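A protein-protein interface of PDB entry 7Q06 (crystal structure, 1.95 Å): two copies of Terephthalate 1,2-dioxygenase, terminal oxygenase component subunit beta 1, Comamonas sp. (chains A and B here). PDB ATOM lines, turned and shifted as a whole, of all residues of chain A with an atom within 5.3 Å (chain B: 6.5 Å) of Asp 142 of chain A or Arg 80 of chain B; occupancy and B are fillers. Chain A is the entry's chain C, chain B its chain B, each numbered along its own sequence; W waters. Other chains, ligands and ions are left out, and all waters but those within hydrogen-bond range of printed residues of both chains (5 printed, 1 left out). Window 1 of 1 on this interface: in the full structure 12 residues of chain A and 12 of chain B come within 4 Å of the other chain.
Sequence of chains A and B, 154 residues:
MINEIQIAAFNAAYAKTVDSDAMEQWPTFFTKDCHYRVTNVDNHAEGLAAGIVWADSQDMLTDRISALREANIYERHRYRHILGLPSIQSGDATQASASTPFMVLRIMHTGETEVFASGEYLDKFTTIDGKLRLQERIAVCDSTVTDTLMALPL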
ATOM      1  N   VAL A  41      16.970  14.917 -22.363  1.00  0.00           N
ATOM      2  CA  VAL A  41      17.312  15.346 -23.736  1.00  0.00           C
ATOM      3  C   VAL A  41      17.508  16.848 -23.793  1.00  0.00           C
ATOM      4  O   VAL A  41      18.405  17.280 -24.546  1.00  0.00           O
ATOM      5  CB  VAL A  41      16.273  14.902 -24.772  1.00  0.00           C
ATOM      6  CG1 VAL A  41      16.328  13.420 -25.021  1.00  0.00           C
ATOM      7  CG2 VAL A  41      14.854  15.313 -24.424  1.00  0.00           C
ATOM      8  N   PRO A 101      19.382   2.018 -25.901  1.00  0.00           N
ATOM      9  CA  PRO A 101      18.041   2.444 -25.571  1.00  0.00           C
ATOM     10  C   PRO A 101      17.553   1.749 -24.301  1.00  0.00           C
ATOM     11  O   PRO A 101      17.876   0.606 -24.092  1.00  0.00           O
ATOM     12  CB  PRO A 101      17.191   1.999 -26.756  1.00  0.00           C
ATOM     13  CG  PRO A 101      18.199   1.851 -27.879  1.00  0.00           C
ATOM     14  CD  PRO A 101      19.431   1.280 -27.188  1.00  0.00           C
ATOM     15  N   PHE A 102      16.719   2.436 -23.519  1.00  0.00           N
ATOM     16  CA  PHE A 102      16.094   1.818 -22.324  1.00  0.00           C
ATOM     17  C   PHE A 102      14.675   2.327 -22.135  1.00  0.00           C
ATOM     18  O   PHE A 102      14.340   3.450 -22.574  1.00  0.00           O
ATOM     19  CB  PHE A 102      16.907   2.075 -21.060  1.00  0.00           C
ATOM     20  CG  PHE A 102      16.951   3.500 -20.567  1.00  0.00           C
ATOM     21  CD1 PHE A 102      15.905   4.026 -19.824  1.00  0.00           C
ATOM     22  CD2 PHE A 102      18.064   4.300 -20.801  1.00  0.00           C
ATOM     23  CE1 PHE A 102      15.937   5.322 -19.357  1.00  0.00           C
ATOM     24  CE2 PHE A 102      18.108   5.596 -20.323  1.00  0.00           C
ATOM     25  CZ  PHE A 102      17.039   6.110 -19.602  1.00  0.00           C
ATOM     26  N   SER A 118      12.311   6.628 -20.024  1.00  0.00           N
ATOM     27  CA  SER A 118      12.860   5.993 -21.248  1.00  0.00           C
ATOM     28  C   SER A 118      13.975   6.883 -21.769  1.00  0.00           C
ATOM     29  O   SER A 118      14.022   8.076 -21.383  1.00  0.00           O
ATOM     30  CB  SER A 118      11.752   5.789 -22.280  1.00  0.00           C
ATOM     31  OG  SER A 118      11.303   7.050 -22.794  1.00  0.00           O
ATOM     32  N   GLY A 119      14.864   6.332 -22.601  1.00  0.00           N
ATOM     33  CA  GLY A 119      15.936   7.162 -23.148  1.00  0.00           C
ATOM     34  C   GLY A 119      17.076   6.308 -23.656  1.00  0.00           C
ATOM     35  O   GLY A 119      16.809   5.183 -24.166  1.00  0.00           O
ATOM     36  N   GLU A 120      18.309   6.800 -23.493  1.00  0.00           N
ATOM     37  CA  GLU A 120      19.475   6.002 -23.897  1.00  0.00           C
ATOM     38  C   GLU A 120      20.537   6.232 -22.853  1.00  0.00           C
ATOM     39  O   GLU A 120      20.680   7.356 -22.333  1.00  0.00           O
ATOM     40  CB  GLU A 120      19.892   6.274 -25.361  1.00  0.00           C
ATOM     41  CG  GLU A 120      20.285   7.692 -25.603  1.00  0.00           C
ATOM     42  CD  GLU A 120      20.689   8.054 -27.036  1.00  0.00           C
ATOM     43  OE1 GLU A 120      20.996   7.167 -27.831  1.00  0.00           O
ATOM     44  OE2 GLU A 120      20.715   9.251 -27.297  1.00  0.00           O
ATOM     45  N   VAL A 140      20.313   9.481 -20.429  1.00  0.00           N
ATOM     46  CA  VAL A 140      19.648  10.652 -21.023  1.00  0.00           C
ATOM     47  C   VAL A 140      18.162  10.294 -21.160  1.00  0.00           C
ATOM     48  O   VAL A 140      17.846   9.517 -22.037  1.00  0.00           O
ATOM     49  CB  VAL A 140      20.277  11.105 -22.347  1.00  0.00           C
ATOM     50  CG1 VAL A 140      19.589  12.366 -22.862  1.00  0.00           C
ATOM     51  CG2 VAL A 140      21.771  11.362 -22.212  1.00  0.00           C
ATOM     52  N   CYS A 141      17.308  10.851 -20.300  1.00  0.00           N
ATOM     53  CA  CYS A 141      15.851  10.559 -20.286  1.00  0.00           C
ATOM     54  C   CYS A 141      15.178  11.324 -21.418  1.00  0.00           C
ATOM     55  O   CYS A 141      15.528  12.529 -21.641  1.00  0.00           O
ATOM     56  CB  CYS A 141      15.204  10.814 -18.922  1.00  0.00           C
ATOM     57  SG  CYS A 141      15.846   9.681 -17.647  1.00  0.00           S
ATOM     58  N   ASP A 142      14.260  10.663 -22.102  1.00  0.00           N
ATOM     59  CA  ASP A 142      13.421  11.285 -23.152  1.00  0.00           C
ATOM     60  C   ASP A 142      12.552  12.407 -22.574  1.00  0.00           C
ATOM     61  O   ASP A 142      12.236  13.379 -23.334  1.00  0.00           O
ATOM     62  CB  ASP A 142      12.571  10.212 -23.842  1.00  0.00           C
ATOM     63  CG  ASP A 142      13.409   9.168 -24.608  1.00  0.00           C
ATOM     64  OD1 ASP A 142      14.401   9.584 -25.199  1.00  0.00           O
ATOM     65  OD2 ASP A 142      13.031   7.948 -24.624  1.00  0.00           O
ATOM     66  N   SER A 143      12.023  12.248 -21.352  1.00  0.00           N
ATOM     67  CA  SER A 143      11.094  13.221 -20.717  1.00  0.00           C
ATOM     68  C   SER A 143      11.887  14.088 -19.716  1.00  0.00           C
ATOM     69  O   SER A 143      12.794  13.562 -19.010  1.00  0.00           O
ATOM     70  CB  SER A 143       9.985  12.522 -20.037  1.00  0.00           C
ATOM     71  OG  SER A 143       9.123  13.429 -19.351  1.00  0.00           O
ATOM     72  N   THR A 144      11.469  15.343 -19.554  1.00  0.00           N
ATOM     73  CA  THR A 144      11.953  16.245 -18.480  1.00  0.00           C
ATOM     74  C   THR A 144      11.187  15.978 -17.174  1.00  0.00           C
ATOM     75  O   THR A 144      11.509  16.637 -16.144  1.00  0.00           O
ATOM     76  CB  THR A 144      11.765  17.698 -18.932  1.00  0.00           C
ATOM     77  OG1 THR A 144      10.384  17.850 -19.284  1.00  0.00           O
ATOM     78  CG2 THR A 144      12.596  17.998 -20.169  1.00  0.00           C
ATOM     79  N   ALA B  15      15.840   1.964 -35.913  1.00  0.00           N
ATOM     80  CA  ALA B  15      15.241   2.595 -34.716  1.00  0.00           C
ATOM     81  C   ALA B  15      16.037   3.835 -34.329  1.00  0.00           C
ATOM     82  O   ALA B  15      15.417   4.873 -34.007  1.00  0.00           O
ATOM     83  CB  ALA B  15      15.150   1.624 -33.544  1.00  0.00           C
ATOM     84  N   LYS B  16      17.346   3.742 -34.291  1.00  0.00           N
ATOM     85  CA  LYS B  16      18.211   4.882 -33.837  1.00  0.00           C
ATOM     86  C   LYS B  16      17.992   6.029 -34.817  1.00  0.00           C
ATOM     87  O   LYS B  16      17.881   7.168 -34.386  1.00  0.00           O
ATOM     88  CB  LYS B  16      19.684   4.472 -33.811  1.00  0.00           C
ATOM     89  CG  LYS B  16      20.645   5.457 -33.180  1.00  0.00           C
ATOM     90  CD  LYS B  16      22.015   4.847 -32.995  1.00  0.00           C
ATOM     91  CE  LYS B  16      22.867   5.594 -31.976  1.00  0.00           C
ATOM     92  NZ  LYS B  16      23.502   6.739 -32.661  1.00  0.00           N
ATOM     93  N   ASP B  19      14.478   7.476 -34.085  1.00  0.00           N
ATOM     94  CA  ASP B  19      14.333   8.025 -32.722  1.00  0.00           C
ATOM     95  C   ASP B  19      15.238   9.249 -32.511  1.00  0.00           C
ATOM     96  O   ASP B  19      14.951  10.009 -31.606  1.00  0.00           O
ATOM     97  CB  ASP B  19      14.638   6.959 -31.690  1.00  0.00           C
ATOM     98  CG  ASP B  19      13.572   5.865 -31.646  1.00  0.00           C
ATOM     99  OD1 ASP B  19      12.535   6.005 -32.359  1.00  0.00           O
ATOM    100  OD2 ASP B  19      13.824   4.900 -30.927  1.00  0.00           O
ATOM    101  N   ARG B  78       9.017  13.082 -29.630  1.00  0.00           N
ATOM    102  CA  ARG B  78       9.997  12.092 -30.095  1.00  0.00           C
ATOM    103  C   ARG B  78       9.410  10.689 -29.896  1.00  0.00           C
ATOM    104  O   ARG B  78       8.507  10.524 -29.059  1.00  0.00           O
ATOM    105  CB  ARG B  78      11.311  12.257 -29.328  1.00  0.00           C
ATOM    106  CG  ARG B  78      12.057  13.544 -29.689  1.00  0.00           C
ATOM    107  CD  ARG B  78      13.528  13.538 -29.224  1.00  0.00           C
ATOM    108  NE  ARG B  78      14.199  14.849 -29.299  1.00  0.00           N
ATOM    109  CZ  ARG B  78      13.930  15.912 -28.508  1.00  0.00           C
ATOM    110  NH1 ARG B  78      14.575  17.061 -28.672  1.00  0.00           N
ATOM    111  NH2 ARG B  78      13.038  15.832 -27.533  1.00  0.00           N
ATOM    112  N   TYR B  79      10.025   9.712 -30.567  1.00  0.00           N
ATOM    113  CA  TYR B  79       9.744   8.279 -30.440  1.00  0.00           C
ATOM    114  C   TYR B  79      10.862   7.613 -29.635  1.00  0.00           C
ATOM    115  O   TYR B  79      12.019   8.010 -29.685  1.00  0.00           O
ATOM    116  CB  TYR B  79       9.640   7.603 -31.804  1.00  0.00           C
ATOM    117  CG  TYR B  79       8.394   7.891 -32.595  1.00  0.00           C
ATOM    118  CD1 TYR B  79       7.271   8.481 -32.045  1.00  0.00           C
ATOM    119  CD2 TYR B  79       8.317   7.471 -33.917  1.00  0.00           C
ATOM    120  CE1 TYR B  79       6.130   8.719 -32.815  1.00  0.00           C
ATOM    121  CE2 TYR B  79       7.180   7.664 -34.683  1.00  0.00           C
ATOM    122  CZ  TYR B  79       6.069   8.288 -34.143  1.00  0.00           C
ATOM    123  OH  TYR B  79       4.981   8.530 -34.954  1.00  0.00           O
ATOM    124  N   ARG B  80      10.488   6.548 -28.939  1.00  0.00           N
ATOM    125  CA  ARG B  80      11.425   5.552 -28.403  1.00  0.00           C
ATOM    126  C   ARG B  80      10.921   4.171 -28.844  1.00  0.00           C
ATOM    127  O   ARG B  80       9.906   3.708 -28.312  1.00  0.00           O
ATOM    128  CB  ARG B  80      11.448   5.688 -26.890  1.00  0.00           C
ATOM    129  CG  ARG B  80      12.375   4.705 -26.172  1.00  0.00           C
ATOM    130  CD  ARG B  80      13.807   4.787 -26.593  1.00  0.00           C
ATOM    131  NE  ARG B  80      14.372   6.136 -26.462  1.00  0.00           N
ATOM    132  CZ  ARG B  80      15.505   6.529 -27.063  1.00  0.00           C
ATOM    133  NH1 ARG B  80      16.167   5.749 -27.912  1.00  0.00           N
ATOM    134  NH2 ARG B  80      15.957   7.725 -26.842  1.00  0.00           N
ATOM    135  N   HIS B  81      11.618   3.560 -29.786  1.00  0.00           N
ATOM    136  CA  HIS B  81      11.416   2.183 -30.268  1.00  0.00           C
ATOM    137  C   HIS B  81      12.049   1.192 -29.313  1.00  0.00           C
ATOM    138  O   HIS B  81      13.215   1.351 -28.975  1.00  0.00           O
ATOM    139  CB  HIS B  81      12.044   2.021 -31.637  1.00  0.00           C
ATOM    140  CG  HIS B  81      11.251   2.621 -32.748  1.00  0.00           C
ATOM    141  ND1 HIS B  81      11.234   3.993 -32.960  1.00  0.00           N
ATOM    142  CD2 HIS B  81      10.557   2.043 -33.759  1.00  0.00           C
ATOM    143  CE1 HIS B  81      10.530   4.234 -34.067  1.00  0.00           C
ATOM    144  NE2 HIS B  81      10.100   3.017 -34.583  1.00  0.00           N
ATOM    145  N   ILE B  82      11.284   0.210 -28.915  1.00  0.00           N
ATOM    146  CA  ILE B  82      11.754  -0.974 -28.164  1.00  0.00           C
ATOM    147  C   ILE B  82      11.359  -2.176 -29.022  1.00  0.00           C
ATOM    148  O   ILE B  82      10.167  -2.334 -29.320  1.00  0.00           O
ATOM    149  CB  ILE B  82      11.122  -1.033 -26.772  1.00  0.00           C
ATOM    150  CG1 ILE B  82      11.366   0.241 -25.973  1.00  0.00           C
ATOM    151  CG2 ILE B  82      11.699  -2.224 -26.048  1.00  0.00           C
ATOM    152  CD1 ILE B  82      12.842   0.468 -25.657  1.00  0.00           C
ATOM    153  N   MET B 103       7.402  -1.954 -30.114  1.00  0.00           N
ATOM    154  CA  MET B 103       6.596  -1.009 -29.342  1.00  0.00           C
ATOM    155  C   MET B 103       7.254   0.361 -29.581  1.00  0.00           C
ATOM    156  O   MET B 103       8.520   0.474 -29.524  1.00  0.00           O
ATOM    157  CB  MET B 103       6.611  -1.393 -27.859  1.00  0.00           C
ATOM    158  CG  MET B 103       5.993  -0.338 -26.953  1.00  0.00           C
ATOM    159  SD  MET B 103       6.241  -0.816 -25.220  1.00  0.00           S
ATOM    160  CE  MET B 103       8.007  -0.606 -25.117  1.00  0.00           C
ATOM    161  N   VAL B 104       6.427   1.389 -29.760  1.00  0.00           N
ATOM    162  CA  VAL B 104       6.899   2.786 -29.854  1.00  0.00           C
ATOM    163  C   VAL B 104       6.270   3.614 -28.737  1.00  0.00           C
ATOM    164  O   VAL B 104       5.041   3.687 -28.681  1.00  0.00           O
ATOM    165  CB  VAL B 104       6.585   3.333 -31.243  1.00  0.00           C
ATOM    166  CG1 VAL B 104       7.020   4.802 -31.375  1.00  0.00           C
ATOM    167  CG2 VAL B 104       7.255   2.474 -32.298  1.00  0.00           C
ATOM    168  N   LEU B 105       7.093   4.191 -27.888  1.00  0.00           N
ATOM    169  CA  LEU B 105       6.658   5.257 -26.963  1.00  0.00           C
ATOM    170  C   LEU B 105       6.673   6.594 -27.712  1.00  0.00           C
ATOM    171  O   LEU B 105       7.626   6.822 -28.522  1.00  0.00           O
ATOM    172  CB  LEU B 105       7.584   5.311 -25.752  1.00  0.00           C
ATOM    173  CG  LEU B 105       7.779   4.021 -24.970  1.00  0.00           C
ATOM    174  CD1 LEU B 105       8.818   4.231 -23.862  1.00  0.00           C
ATOM    175  CD2 LEU B 105       6.490   3.525 -24.405  1.00  0.00           C
ATOM    176  N   ARG B 106       5.676   7.444 -27.432  1.00  0.00           N
ATOM    177  CA  ARG B 106       5.725   8.871 -27.791  1.00  0.00           C
ATOM    178  C   ARG B 106       5.981   9.695 -26.539  1.00  0.00           C
ATOM    179  O   ARG B 106       5.279   9.498 -25.543  1.00  0.00           O
ATOM    180  CB  ARG B 106       4.464   9.315 -28.504  1.00  0.00           C
ATOM    181  CG  ARG B 106       4.481  10.794 -28.889  1.00  0.00           C
ATOM    182  CD  ARG B 106       3.179  11.219 -29.552  1.00  0.00           C
ATOM    183  NE  ARG B 106       2.121  11.159 -28.584  1.00  0.00           N
ATOM    184  CZ  ARG B 106       0.819  11.153 -28.851  1.00  0.00           C
ATOM    185  NH1 ARG B 106      -0.030  11.178 -27.836  1.00  0.00           N
ATOM    186  NH2 ARG B 106       0.353  11.272 -30.084  1.00  0.00           N
ATOM    187  N   ILE B 107       7.011  10.532 -26.608  1.00  0.00           N
ATOM    188  CA  ILE B 107       7.302  11.512 -25.536  1.00  0.00           C
ATOM    189  C   ILE B 107       7.055  12.915 -26.100  1.00  0.00           C
ATOM    190  O   ILE B 107       7.812  13.342 -26.972  1.00  0.00           O
ATOM    191  CB  ILE B 107       8.716  11.314 -24.977  1.00  0.00           C
ATOM    192  CG1 ILE B 107       8.978   9.853 -24.575  1.00  0.00           C
ATOM    193  CG2 ILE B 107       8.925  12.233 -23.771  1.00  0.00           C
ATOM    194  CD1 ILE B 107       9.577   9.005 -25.673  1.00  0.00           C
ATOM    195  N   MET B 108       6.054  13.596 -25.582  1.00  0.00           N
ATOM    196  CA  MET B 108       5.772  15.001 -25.955  1.00  0.00           C
ATOM    197  C   MET B 108       6.893  15.882 -25.392  1.00  0.00           C
ATOM    198  O   MET B 108       7.464  15.540 -24.318  1.00  0.00           O
ATOM    199  CB  MET B 108       4.410  15.460 -25.435  1.00  0.00           C
ATOM    200  CG  MET B 108       3.210  14.626 -25.871  1.00  0.00           C
ATOM    201  SD  MET B 108       3.107  14.480 -27.717  1.00  0.00           S
ATOM    202  CE  MET B 108       2.824  16.154 -28.279  1.00  0.00           C
ATOM    203  N   GLY B 111       6.530  16.410 -21.784  1.00  0.00           N
ATOM    204  CA  GLY B 111       6.982  15.376 -20.840  1.00  0.00           C
ATOM    205  C   GLY B 111       6.134  14.116 -20.778  1.00  0.00           C
ATOM    206  O   GLY B 111       6.666  13.132 -20.223  1.00  0.00           O
ATOM    207  N   THR B 113       4.655  10.589 -21.549  1.00  0.00           N
ATOM    208  CA  THR B 113       5.117   9.355 -22.221  1.00  0.00           C
ATOM    209  C   THR B 113       3.896   8.445 -22.372  1.00  0.00           C
ATOM    210  O   THR B 113       3.220   8.227 -21.375  1.00  0.00           O
ATOM    211  CB  THR B 113       6.241   8.660 -21.452  1.00  0.00           C
ATOM    212  OG1 THR B 113       7.281   9.618 -21.279  1.00  0.00           O
ATOM    213  CG2 THR B 113       6.724   7.434 -22.195  1.00  0.00           C
HETATM  214  O   HOH W   1      10.838  15.631 -24.066  1.00  0.00           O
HETATM  215  O   HOH W   2      10.022   8.801 -21.111  1.00  0.00           O
HETATM  216  O   HOH W   3      12.377  13.334 -26.167  1.00  0.00           O
HETATM  217  O   HOH W   4       9.768  16.508 -21.889  1.00  0.00           O
HETATM  218  O   HOH W   5      18.462   5.720 -29.645  1.00  0.00           O
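Of chain A, only Gly 119 (3.5 Å) and Asp 142 (2.9 Å) come within 4 Å of Arg 80 of chain B. Of the printed residues of chain B, Ser 143 of chain A touches Ile 107 (3.9 Å) and Gly 111 (2.6 Å). Printed residues of chain B within 4 Å of Ser 118 of chain A: Leu 105 (3.7 Å) and Ile 107 (3.9 Å). Ala 15 of chain B touches none of the printed residues of chain A. The nearest residue of chain A that does not touch Arg 80 of chain B is Pro 101 of chain A (4.1 Å).
Among the printed residues, pairs that only touch across the chains: Asp 142 of chain A with Ile 107 of chain B (3.5 Å), Val 41 of chain A with Arg 78 of chain B (3.6 Å), Ser 118 of chain A with Leu 105 of chain B (3.7 Å), Ser 143 of chain A with Ile 107 of chain B (3.9 Å) and Ser 118 of chain A with Ile 107 of chain B (3.9 Å).
Hydrophobic or aromatic side chains of chain A within 4 Å of the printed part of chain B: Val 41. Along chain A the printed residues that touch a printed residue of chain B span positions 41 to 143. Hydrophobic or aromatic side chains of chain B that line the printed part of chain A: Leu 105 and Ile 107. Among the printed residues, Asp or Glu carboxylates within 4 Å of a Lys or Arg side-chain nitrogen of the other chain: Asp 142 of chain A with Arg 80 of chain B.
No position is printed for both chains. Of the 8 pairs that touch across the chains among the printed residues, none has its exchanged pair printed and touching as well.
NH1 of Arg 80 of chain B is in salt-bridge range of OD2 of Asp 19 of chain B (3.9 Å). N of Ile 107 of chain B lies within hydrogen-bond range of O of Arg 78 of chain B, 2.9 Å away. O of Arg 80 of chain B sits at hydrogen-bond distance from N of Leu 105 of chain B, 2.9 Å away. The backbone NH (N) of Val 41 of chain A is in hydrogen-bond range of the backbone carbonyl oxygen (O) of Cys 141 of chain A (2.9 Å). OG of Ser 118 of chain A sits at hydrogen-bond distance from OD2 of Asp 142 of chain A (2.7 Å). OD2 of Asp 142 of chain A lies within hydrogen-bond range of N of Gly 119 of chain A, 3.2 Å away.
The guanidinium group of Arg 80 of chain B lies close to the backbone carbonyl oxygen of Gly 119 of chain A, at 3.5 Å. NE of Arg 80 of chain B lies within salt-bridge range of OD2 of Asp 142 of chain A (2.9 Å). O of Gly 111 of chain B sits at hydrogen-bond distance from OG of Ser 143 of chain A (2.6 Å).
Water W2 lies within hydrogen-bond range of the side-chain hydroxyl of Ser 118 of chain A and the side-chain hydroxyl of Thr 113 of chain B. Water W1 bridges the backbone carbonyl oxygen (O) of Asp 142 of chain A (2.7 Å) and the backbone carbonyl oxygen (O) of Met 108 of chain B (3.4 Å). Water W3 lies within hydrogen-bond range of O of Asp 142 of chain A (2.8 Å) and NH2 of Arg 78 of chain B (2.9 Å). Water W5 lies within hydrogen-bond range of NH1 of Arg 80 of chain B (2.9 Å) and OE1 of Glu 120 of chain A (3.4 Å). Water W4 lies within hydrogen-bond range of the side-chain hydroxyl (OG1) of Thr 144 of chain A, the backbone NH (N) of Gly 111 of chain B and the backbone carbonyl oxygen (O) of Met 108 of chain B.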
